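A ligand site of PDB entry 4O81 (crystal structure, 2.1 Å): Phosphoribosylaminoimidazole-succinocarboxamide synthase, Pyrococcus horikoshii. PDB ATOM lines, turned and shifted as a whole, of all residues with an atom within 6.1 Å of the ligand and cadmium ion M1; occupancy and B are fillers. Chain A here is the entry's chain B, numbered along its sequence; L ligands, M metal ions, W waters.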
ATOM      1  N   ALA A  12      12.780 -24.456   4.055  1.00  0.00           N
ATOM      2  CA  ALA A  12      12.412 -25.572   4.977  1.00  0.00           C
ATOM      3  C   ALA A  12      12.809 -25.268   6.419  1.00  0.00           C
ATOM      4  O   ALA A  12      12.498 -26.039   7.340  1.00  0.00           O
ATOM      5  CB  ALA A  12      13.030 -26.893   4.499  1.00  0.00           C
ATOM      6  N   LYS A  13      13.505 -24.142   6.617  1.00  0.00           N
ATOM      7  CA  LYS A  13      13.751 -23.607   7.965  1.00  0.00           C
ATOM      8  C   LYS A  13      13.425 -22.114   8.031  1.00  0.00           C
ATOM      9  O   LYS A  13      13.607 -21.384   7.061  1.00  0.00           O
ATOM     10  CB  LYS A  13      15.208 -23.829   8.418  1.00  0.00           C
ATOM     11  CG  LYS A  13      15.670 -25.271   8.493  1.00  0.00           C
ATOM     12  CD  LYS A  13      16.940 -25.434   9.319  1.00  0.00           C
ATOM     13  CE  LYS A  13      18.149 -24.715   8.724  1.00  0.00           C
ATOM     14  NZ  LYS A  13      18.646 -25.346   7.474  1.00  0.00           N
ATOM     15  N   LYS A  14      12.944 -21.679   9.191  1.00  0.00           N
ATOM     16  CA  LYS A  14      12.784 -20.255   9.466  1.00  0.00           C
ATOM     17  C   LYS A  14      13.750 -19.894  10.590  1.00  0.00           C
ATOM     18  O   LYS A  14      13.817 -20.603  11.602  1.00  0.00           O
ATOM     19  CB  LYS A  14      11.349 -19.922   9.854  1.00  0.00           C
ATOM     20  N   MET A  15      14.525 -18.828  10.388  1.00  0.00           N
ATOM     21  CA  MET A  15      15.482 -18.379  11.411  1.00  0.00           C
ATOM     22  C   MET A  15      14.921 -17.158  12.069  1.00  0.00           C
ATOM     23  O   MET A  15      14.854 -16.091  11.456  1.00  0.00           O
ATOM     24  CB  MET A  15      16.871 -18.052  10.842  1.00  0.00           C
ATOM     25  CG  MET A  15      17.447 -19.131   9.930  1.00  0.00           C
ATOM     26  SD  MET A  15      17.715 -20.863  10.873  1.00  0.00           S
ATOM     27  CE  MET A  15      19.391 -20.375  11.786  1.00  0.00           C
ATOM     28  N   LEU A  23      19.396 -17.267  18.360  1.00  0.00           N
ATOM     29  CA  LEU A  23      18.226 -17.315  17.489  1.00  0.00           C
ATOM     30  C   LEU A  23      17.500 -18.661  17.536  1.00  0.00           C
ATOM     31  O   LEU A  23      18.008 -19.626  18.097  1.00  0.00           O
ATOM     32  CB  LEU A  23      18.600 -16.903  16.068  1.00  0.00           C
ATOM     33  CG  LEU A  23      19.427 -17.863  15.226  1.00  0.00           C
ATOM     34  CD1 LEU A  23      18.488 -18.576  14.268  1.00  0.00           C
ATOM     35  CD2 LEU A  23      20.502 -17.124  14.464  1.00  0.00           C
ATOM     36  N   MET A  25      15.856 -21.640  15.308  1.00  0.00           N
ATOM     37  CA  MET A  25      15.805 -22.309  14.014  1.00  0.00           C
ATOM     38  C   MET A  25      14.553 -23.143  14.034  1.00  0.00           C
ATOM     39  O   MET A  25      14.423 -24.102  14.797  1.00  0.00           O
ATOM     40  CB  MET A  25      17.096 -23.128  13.910  1.00  0.00           C
ATOM     41  CG  MET A  25      17.142 -24.032  12.675  1.00  0.00           C
ATOM     42  SD  MET A  25      19.008 -24.585  12.310  1.00  0.00           S
ATOM     43  CE  MET A  25      19.286 -25.791  13.840  1.00  0.00           C
ATOM     44  N   HIS A  68      26.614 -24.801  17.141  1.00  0.00           N
ATOM     45  CA  HIS A  68      25.722 -23.693  17.486  1.00  0.00           C
ATOM     46  C   HIS A  68      24.542 -24.095  18.351  1.00  0.00           C
ATOM     47  O   HIS A  68      23.781 -23.224  18.798  1.00  0.00           O
ATOM     48  CB  HIS A  68      25.263 -22.981  16.220  1.00  0.00           C
ATOM     49  CG  HIS A  68      24.259 -23.766  15.390  1.00  0.00           C
ATOM     50  ND1 HIS A  68      23.397 -23.147  14.569  1.00  0.00           N
ATOM     51  CD2 HIS A  68      24.025 -25.125  15.267  1.00  0.00           C
ATOM     52  CE1 HIS A  68      22.642 -24.073  13.937  1.00  0.00           C
ATOM     53  NE2 HIS A  68      23.030 -25.279  14.375  1.00  0.00           N
ATOM     54  N   VAL A  80      19.695 -21.730  18.845  1.00  0.00           N
ATOM     55  CA  VAL A  80      21.089 -21.798  18.406  1.00  0.00           C
ATOM     56  C   VAL A  80      21.795 -20.476  18.614  1.00  0.00           C
ATOM     57  O   VAL A  80      21.156 -19.421  18.628  1.00  0.00           O
ATOM     58  CB  VAL A  80      21.224 -22.265  16.934  1.00  0.00           C
ATOM     59  CG1 VAL A  80      20.701 -23.679  16.760  1.00  0.00           C
ATOM     60  CG2 VAL A  80      20.502 -21.315  15.991  1.00  0.00           C
ATOM     61  N   GLU A  81      23.117 -20.519  18.796  1.00  0.00           N
ATOM     62  CA  GLU A  81      23.869 -19.279  18.945  1.00  0.00           C
ATOM     63  C   GLU A  81      24.075 -18.617  17.593  1.00  0.00           C
ATOM     64  O   GLU A  81      24.295 -19.294  16.584  1.00  0.00           O
ATOM     65  CB  GLU A  81      25.175 -19.494  19.722  1.00  0.00           C
ATOM     66  CG  GLU A  81      26.315 -20.122  18.964  1.00  0.00           C
ATOM     67  CD  GLU A  81      27.635 -19.976  19.724  1.00  0.00           C
ATOM     68  OE1 GLU A  81      28.308 -21.009  19.972  1.00  0.00           O
ATOM     69  OE2 GLU A  81      28.002 -18.833  20.074  1.00  0.00           O
ATOM     70  N   LYS A  82      23.959 -17.285  17.574  1.00  0.00           N
ATOM     71  CA  LYS A  82      24.080 -16.548  16.325  1.00  0.00           C
ATOM     72  C   LYS A  82      25.542 -16.470  15.925  1.00  0.00           C
ATOM     73  O   LYS A  82      26.410 -16.171  16.753  1.00  0.00           O
ATOM     74  CB  LYS A  82      23.451 -15.155  16.425  1.00  0.00           C
ATOM     75  CG  LYS A  82      23.116 -14.548  15.068  1.00  0.00           C
ATOM     76  CD  LYS A  82      22.303 -13.261  15.182  1.00  0.00           C
ATOM     77  CE  LYS A  82      23.193 -12.026  15.272  1.00  0.00           C
ATOM     78  NZ  LYS A  82      22.430 -10.876  15.845  1.00  0.00           N
ATOM     79  N   LEU A  83      25.805 -16.769  14.660  1.00  0.00           N
ATOM     80  CA  LEU A  83      27.164 -16.774  14.161  1.00  0.00           C
ATOM     81  C   LEU A  83      27.318 -15.862  12.961  1.00  0.00           C
ATOM     82  O   LEU A  83      26.348 -15.566  12.259  1.00  0.00           O
ATOM     83  CB  LEU A  83      27.595 -18.203  13.761  1.00  0.00           C
ATOM     84  CG  LEU A  83      27.586 -19.302  14.825  1.00  0.00           C
ATOM     85  CD1 LEU A  83      27.844 -20.649  14.148  1.00  0.00           C
ATOM     86  CD2 LEU A  83      28.608 -19.049  15.908  1.00  0.00           C
ATOM     87  N   ASP A  84      28.542 -15.424  12.756  1.00  0.00           N
ATOM     88  CA  ASP A  84      28.974 -14.793  11.534  1.00  0.00           C
ATOM     89  C   ASP A  84      29.329 -15.907  10.517  1.00  0.00           C
ATOM     90  O   ASP A  84      30.396 -16.512  10.609  1.00  0.00           O
ATOM     91  CB  ASP A  84      30.187 -13.913  11.844  1.00  0.00           C
ATOM     92  CG  ASP A  84      30.671 -13.131  10.661  1.00  0.00           C
ATOM     93  OD1 ASP A  84      29.855 -12.838   9.764  1.00  0.00           O
ATOM     94  OD2 ASP A  84      31.866 -12.799  10.646  1.00  0.00           O
ATOM     95  N   MET A  85      28.428 -16.185   9.579  1.00  0.00           N
ATOM     96  CA  MET A  85      28.536 -17.393   8.746  1.00  0.00           C
ATOM     97  C   MET A  85      29.586 -17.255   7.661  1.00  0.00           C
ATOM     98  O   MET A  85      29.742 -16.203   7.062  1.00  0.00           O
ATOM     99  CB  MET A  85      27.213 -17.746   8.056  1.00  0.00           C
ATOM    100  CG  MET A  85      26.072 -18.079   9.038  1.00  0.00           C
ATOM    101  SD  MET A  85      26.482 -19.691  10.102  1.00  0.00           S
ATOM    102  CE  MET A  85      26.499 -20.958   8.599  1.00  0.00           C
ATOM    103  N   TYR A  86      30.308 -18.342   7.415  1.00  0.00           N
ATOM    104  CA  TYR A  86      31.102 -18.438   6.202  1.00  0.00           C
ATOM    105  C   TYR A  86      30.153 -18.719   5.021  1.00  0.00           C
ATOM    106  O   TYR A  86      29.237 -19.513   5.159  1.00  0.00           O
ATOM    107  CB  TYR A  86      32.133 -19.555   6.307  1.00  0.00           C
ATOM    108  CG  TYR A  86      33.251 -19.266   7.276  1.00  0.00           C
ATOM    109  CD1 TYR A  86      34.352 -18.505   6.883  1.00  0.00           C
ATOM    110  CD2 TYR A  86      33.218 -19.782   8.580  1.00  0.00           C
ATOM    111  CE1 TYR A  86      35.396 -18.255   7.759  1.00  0.00           C
ATOM    112  CE2 TYR A  86      34.267 -19.536   9.464  1.00  0.00           C
ATOM    113  CZ  TYR A  86      35.350 -18.775   9.043  1.00  0.00           C
ATOM    114  OH  TYR A  86      36.397 -18.503   9.879  1.00  0.00           O
ATOM    115  N   LYS A 122      28.324 -20.419  -1.366  1.00  0.00           N
ATOM    116  CA  LYS A 122      26.882 -20.374  -1.116  1.00  0.00           C
ATOM    117  C   LYS A 122      26.310 -19.147  -1.806  1.00  0.00           C
ATOM    118  O   LYS A 122      26.461 -18.036  -1.333  1.00  0.00           O
ATOM    119  CB  LYS A 122      26.596 -20.399   0.397  1.00  0.00           C
ATOM    120  CG  LYS A 122      25.245 -20.985   0.765  1.00  0.00           C
ATOM    121  CD  LYS A 122      25.008 -21.007   2.277  1.00  0.00           C
ATOM    122  CE  LYS A 122      23.776 -21.823   2.616  1.00  0.00           C
ATOM    123  NZ  LYS A 122      22.492 -21.099   2.421  1.00  0.00           N
ATOM    124  N   ASP A 124      22.895 -18.406  -4.511  1.00  0.00           N
ATOM    125  CA  ASP A 124      21.742 -18.972  -5.225  1.00  0.00           C
ATOM    126  C   ASP A 124      21.783 -18.674  -6.716  1.00  0.00           C
ATOM    127  O   ASP A 124      21.443 -19.523  -7.538  1.00  0.00           O
ATOM    128  CB  ASP A 124      20.419 -18.467  -4.630  1.00  0.00           C
ATOM    129  CG  ASP A 124      20.102 -19.072  -3.271  1.00  0.00           C
ATOM    130  OD1 ASP A 124      20.405 -20.265  -3.071  1.00  0.00           O
ATOM    131  OD2 ASP A 124      19.519 -18.360  -2.413  1.00  0.00           O
ATOM    132  N   LYS A 175      26.323 -32.213   3.665  1.00  0.00           N
ATOM    133  CA  LYS A 175      26.737 -30.799   3.646  1.00  0.00           C
ATOM    134  C   LYS A 175      26.759 -30.245   5.074  1.00  0.00           C
ATOM    135  O   LYS A 175      25.861 -30.498   5.853  1.00  0.00           O
ATOM    136  CB  LYS A 175      25.806 -29.930   2.770  1.00  0.00           C
ATOM    137  CG  LYS A 175      25.974 -28.407   2.996  1.00  0.00           C
ATOM    138  CD  LYS A 175      24.728 -27.574   2.696  1.00  0.00           C
ATOM    139  CE  LYS A 175      23.523 -27.892   3.583  1.00  0.00           C
ATOM    140  NZ  LYS A 175      23.279 -26.913   4.693  1.00  0.00           N
ATOM    141  N   GLU A 177      27.669 -26.474   7.332  1.00  0.00           N
ATOM    142  CA  GLU A 177      27.934 -25.041   7.284  1.00  0.00           C
ATOM    143  C   GLU A 177      28.595 -24.591   8.598  1.00  0.00           C
ATOM    144  O   GLU A 177      28.370 -25.201   9.670  1.00  0.00           O
ATOM    145  CB  GLU A 177      26.640 -24.258   6.986  1.00  0.00           C
ATOM    146  CG  GLU A 177      25.992 -24.662   5.665  1.00  0.00           C
ATOM    147  CD  GLU A 177      24.830 -23.776   5.255  1.00  0.00           C
ATOM    148  OE1 GLU A 177      24.694 -22.677   5.827  1.00  0.00           O
ATOM    149  OE2 GLU A 177      24.058 -24.172   4.357  1.00  0.00           O
ATOM    150  N   ALA A 189      27.348 -25.106  12.299  1.00  0.00           N
ATOM    151  CA  ALA A 189      26.024 -24.485  12.316  1.00  0.00           C
ATOM    152  C   ALA A 189      24.967 -25.223  11.478  1.00  0.00           C
ATOM    153  O   ALA A 189      25.103 -26.422  11.223  1.00  0.00           O
ATOM    154  CB  ALA A 189      26.138 -23.039  11.852  1.00  0.00           C
ATOM    155  N   ASP A 190      23.942 -24.475  11.053  1.00  0.00           N
ATOM    156  CA  ASP A 190      22.829 -24.954  10.210  1.00  0.00           C
ATOM    157  C   ASP A 190      22.161 -26.228  10.774  1.00  0.00           C
ATOM    158  O   ASP A 190      21.836 -26.279  11.977  1.00  0.00           O
ATOM    159  CB  ASP A 190      23.290 -25.118   8.746  1.00  0.00           C
ATOM    160  CG  ASP A 190      22.132 -25.152   7.772  1.00  0.00           C
ATOM    161  OD1 ASP A 190      21.957 -26.178   7.077  1.00  0.00           O
ATOM    162  OD2 ASP A 190      21.380 -24.147   7.710  1.00  0.00           O
ATOM    163  N   GLU A 191      21.961 -27.249   9.943  1.00  0.00           N
ATOM    164  CA  GLU A 191      21.297 -28.472  10.392  1.00  0.00           C
ATOM    165  C   GLU A 191      22.093 -29.682   9.972  1.00  0.00           C
ATOM    166  O   GLU A 191      22.971 -29.578   9.111  1.00  0.00           O
ATOM    167  CB  GLU A 191      19.865 -28.572   9.827  1.00  0.00           C
ATOM    168  CG  GLU A 191      19.811 -28.874   8.336  1.00  0.00           C
ATOM    169  CD  GLU A 191      18.426 -28.907   7.766  1.00  0.00           C
ATOM    170  OE1 GLU A 191      17.699 -29.899   8.006  1.00  0.00           O
ATOM    171  OE2 GLU A 191      18.067 -27.960   7.056  1.00  0.00           O
ATOM    172  N   THR A 196      20.001 -32.823   4.472  1.00  0.00           N
ATOM    173  CA  THR A 196      21.357 -32.326   4.170  1.00  0.00           C
ATOM    174  C   THR A 196      22.424 -33.441   4.089  1.00  0.00           C
ATOM    175  O   THR A 196      23.625 -33.168   3.962  1.00  0.00           O
ATOM    176  CB  THR A 196      21.822 -31.274   5.207  1.00  0.00           C
ATOM    177  OG1 THR A 196      21.782 -31.860   6.517  1.00  0.00           O
ATOM    178  CG2 THR A 196      20.918 -30.030   5.172  1.00  0.00           C
HETATM  179  P1  LIG L   1      18.726 -21.254   2.809  1.00  0.00           P
HETATM  180  O1  LIG L   1      18.927 -19.846   2.286  1.00  0.00           O
HETATM  181  O2  LIG L   1      20.017 -22.050   2.922  1.00  0.00           O
HETATM  182  O3  LIG L   1      17.586 -22.011   2.177  1.00  0.00           O
HETATM  183  P2  LIG L   1      17.705 -22.177   5.285  1.00  0.00           P
HETATM  184  O4  LIG L   1      16.450 -21.676   5.965  1.00  0.00           O
HETATM  185  O5  LIG L   1      17.669 -23.491   4.557  1.00  0.00           O
HETATM  186  O6  LIG L   1      18.252 -21.000   4.329  1.00  0.00           O
HETATM  187  O7  LIG L   1      18.880 -22.220   6.386  1.00  0.00           O
HETATM  188  C1  LIG L   1      18.925 -21.243   7.414  1.00  0.00           C
HETATM  189  C2  LIG L   1      19.867 -20.085   7.086  1.00  0.00           C
HETATM  190  O8  LIG L   1      20.491 -19.627   8.285  1.00  0.00           O
HETATM  191  C3  LIG L   1      21.001 -20.421   6.144  1.00  0.00           C
HETATM  192  O9  LIG L   1      21.249 -19.247   5.351  1.00  0.00           O
HETATM  193  C4  LIG L   1      22.202 -20.659   7.048  1.00  0.00           C
HETATM  194  O10 LIG L   1      23.430 -20.342   6.390  1.00  0.00           O
HETATM  195  C5  LIG L   1      21.924 -19.713   8.185  1.00  0.00           C
HETATM  196  N1  LIG L   1      22.367 -20.190   9.498  1.00  0.00           N
HETATM  197  C6  LIG L   1      22.333 -21.450   9.951  1.00  0.00           C
HETATM  198  N2  LIG L   1      22.790 -21.522  11.218  1.00  0.00           N
HETATM  199  C7  LIG L   1      23.125 -20.272  11.594  1.00  0.00           C
HETATM  200  C8  LIG L   1      23.674 -19.623  12.812  1.00  0.00           C
HETATM  201  N3  LIG L   1      23.977 -20.333  13.915  1.00  0.00           N
HETATM  202  N4  LIG L   1      23.882 -18.291  12.782  1.00  0.00           N
HETATM  203  C9  LIG L   1      23.581 -17.549  11.695  1.00  0.00           C
HETATM  204  N5  LIG L   1      23.077 -18.063  10.562  1.00  0.00           N
HETATM  205  C10 LIG L   1      22.842 -19.400  10.464  1.00  0.00           C
HETATM  206 CD    CD M   1      19.887 -24.326   3.703  1.00  0.00          CD
HETATM  207 CD    CD M   2      19.515 -26.382   1.375  1.00  0.00          CD
HETATM  208 CD    CD M   3      22.372 -22.751  -1.927  1.00  0.00          CD
HETATM  209  O   HOH W   1      26.262 -20.255   5.031  1.00  0.00           O
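O1 of the ligand lies within salt-bridge range of NZ of Lys 122, at 3.8 Å.
OE1 of Glu 177 is in hydrogen-bond range of O10 of the ligand (2.7 Å).
A nitrogen (N3) of the ligand lies within hydrogen-bond range of the backbone carbonyl oxygen of Glu 81, 2.9 Å away.
ND1 of His 68 sits at hydrogen-bond distance from N3 of the ligand.
O4 of the ligand sits close to O of Lys 13 (3.1 Å).
The side-chain amino group (NZ) of Lys 13 sits at hydrogen-bond distance from an oxygen (O7) of the ligand.
N of Leu 83 lies within hydrogen-bond range of N4 of the ligand (3.1 Å).
The backbone NH of Asp 190 lies within hydrogen-bond range of a nitrogen (N2) of the ligand (3.2 Å).
The side-chain amino group (NZ) of Lys 122 is in salt-bridge range of the side-chain carboxylate (OE2) of Glu 177.
N of Ala 189 is in hydrogen-bond range of O of Glu 177, 2.8 Å away.
The side-chain carboxylate (OE2) of Glu 177 is in salt-bridge range of the side-chain amino group (NZ) of Lys 175 (2.9 Å).
O of His 68 lies within hydrogen-bond range of N of Glu 81 (2.8 Å).
NE2 of His 68 lies within hydrogen-bond range of O of Asp 190 (2.9 Å).
NZ of Lys 13 lies within salt-bridge range of OD2 of Asp 190 (3.0 Å).
The side-chain amino group of Lys 13 lies within salt-bridge range of the side-chain carboxylate of Glu 191 (2.7 Å).
The side-chain carboxylate (OD1) of Asp 190 lies within salt-bridge range of the side-chain amino group (NZ) of Lys 175 (2.8 Å).
CG of Met 15 touches O8 of the ligand, at 3.5 Å.
Leu 23 touches the ligand.
Lys 82 touches the ligand (CA to N4, 3.95 Å).
CG of Met 85 touches N5 of the ligand, at 3.4 Å.
CB of Ala 189 touches N2 of the ligand, at 3.7 Å.
The nearest printed residue that does not touch the ligand is Val 80 (4.2 Å).
No residue comes within 4 Å of cadmium ion M1.
Cadmium ion M1 is bound by an oxygen (O2) of the ligand and an oxygen (O5) of the ligand.
Water W1 lies within hydrogen-bond range of OE1 of Glu 177 (3.0 Å), O of Tyr 86 (3.1 Å) and O10 of the ligand (3.1 Å).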
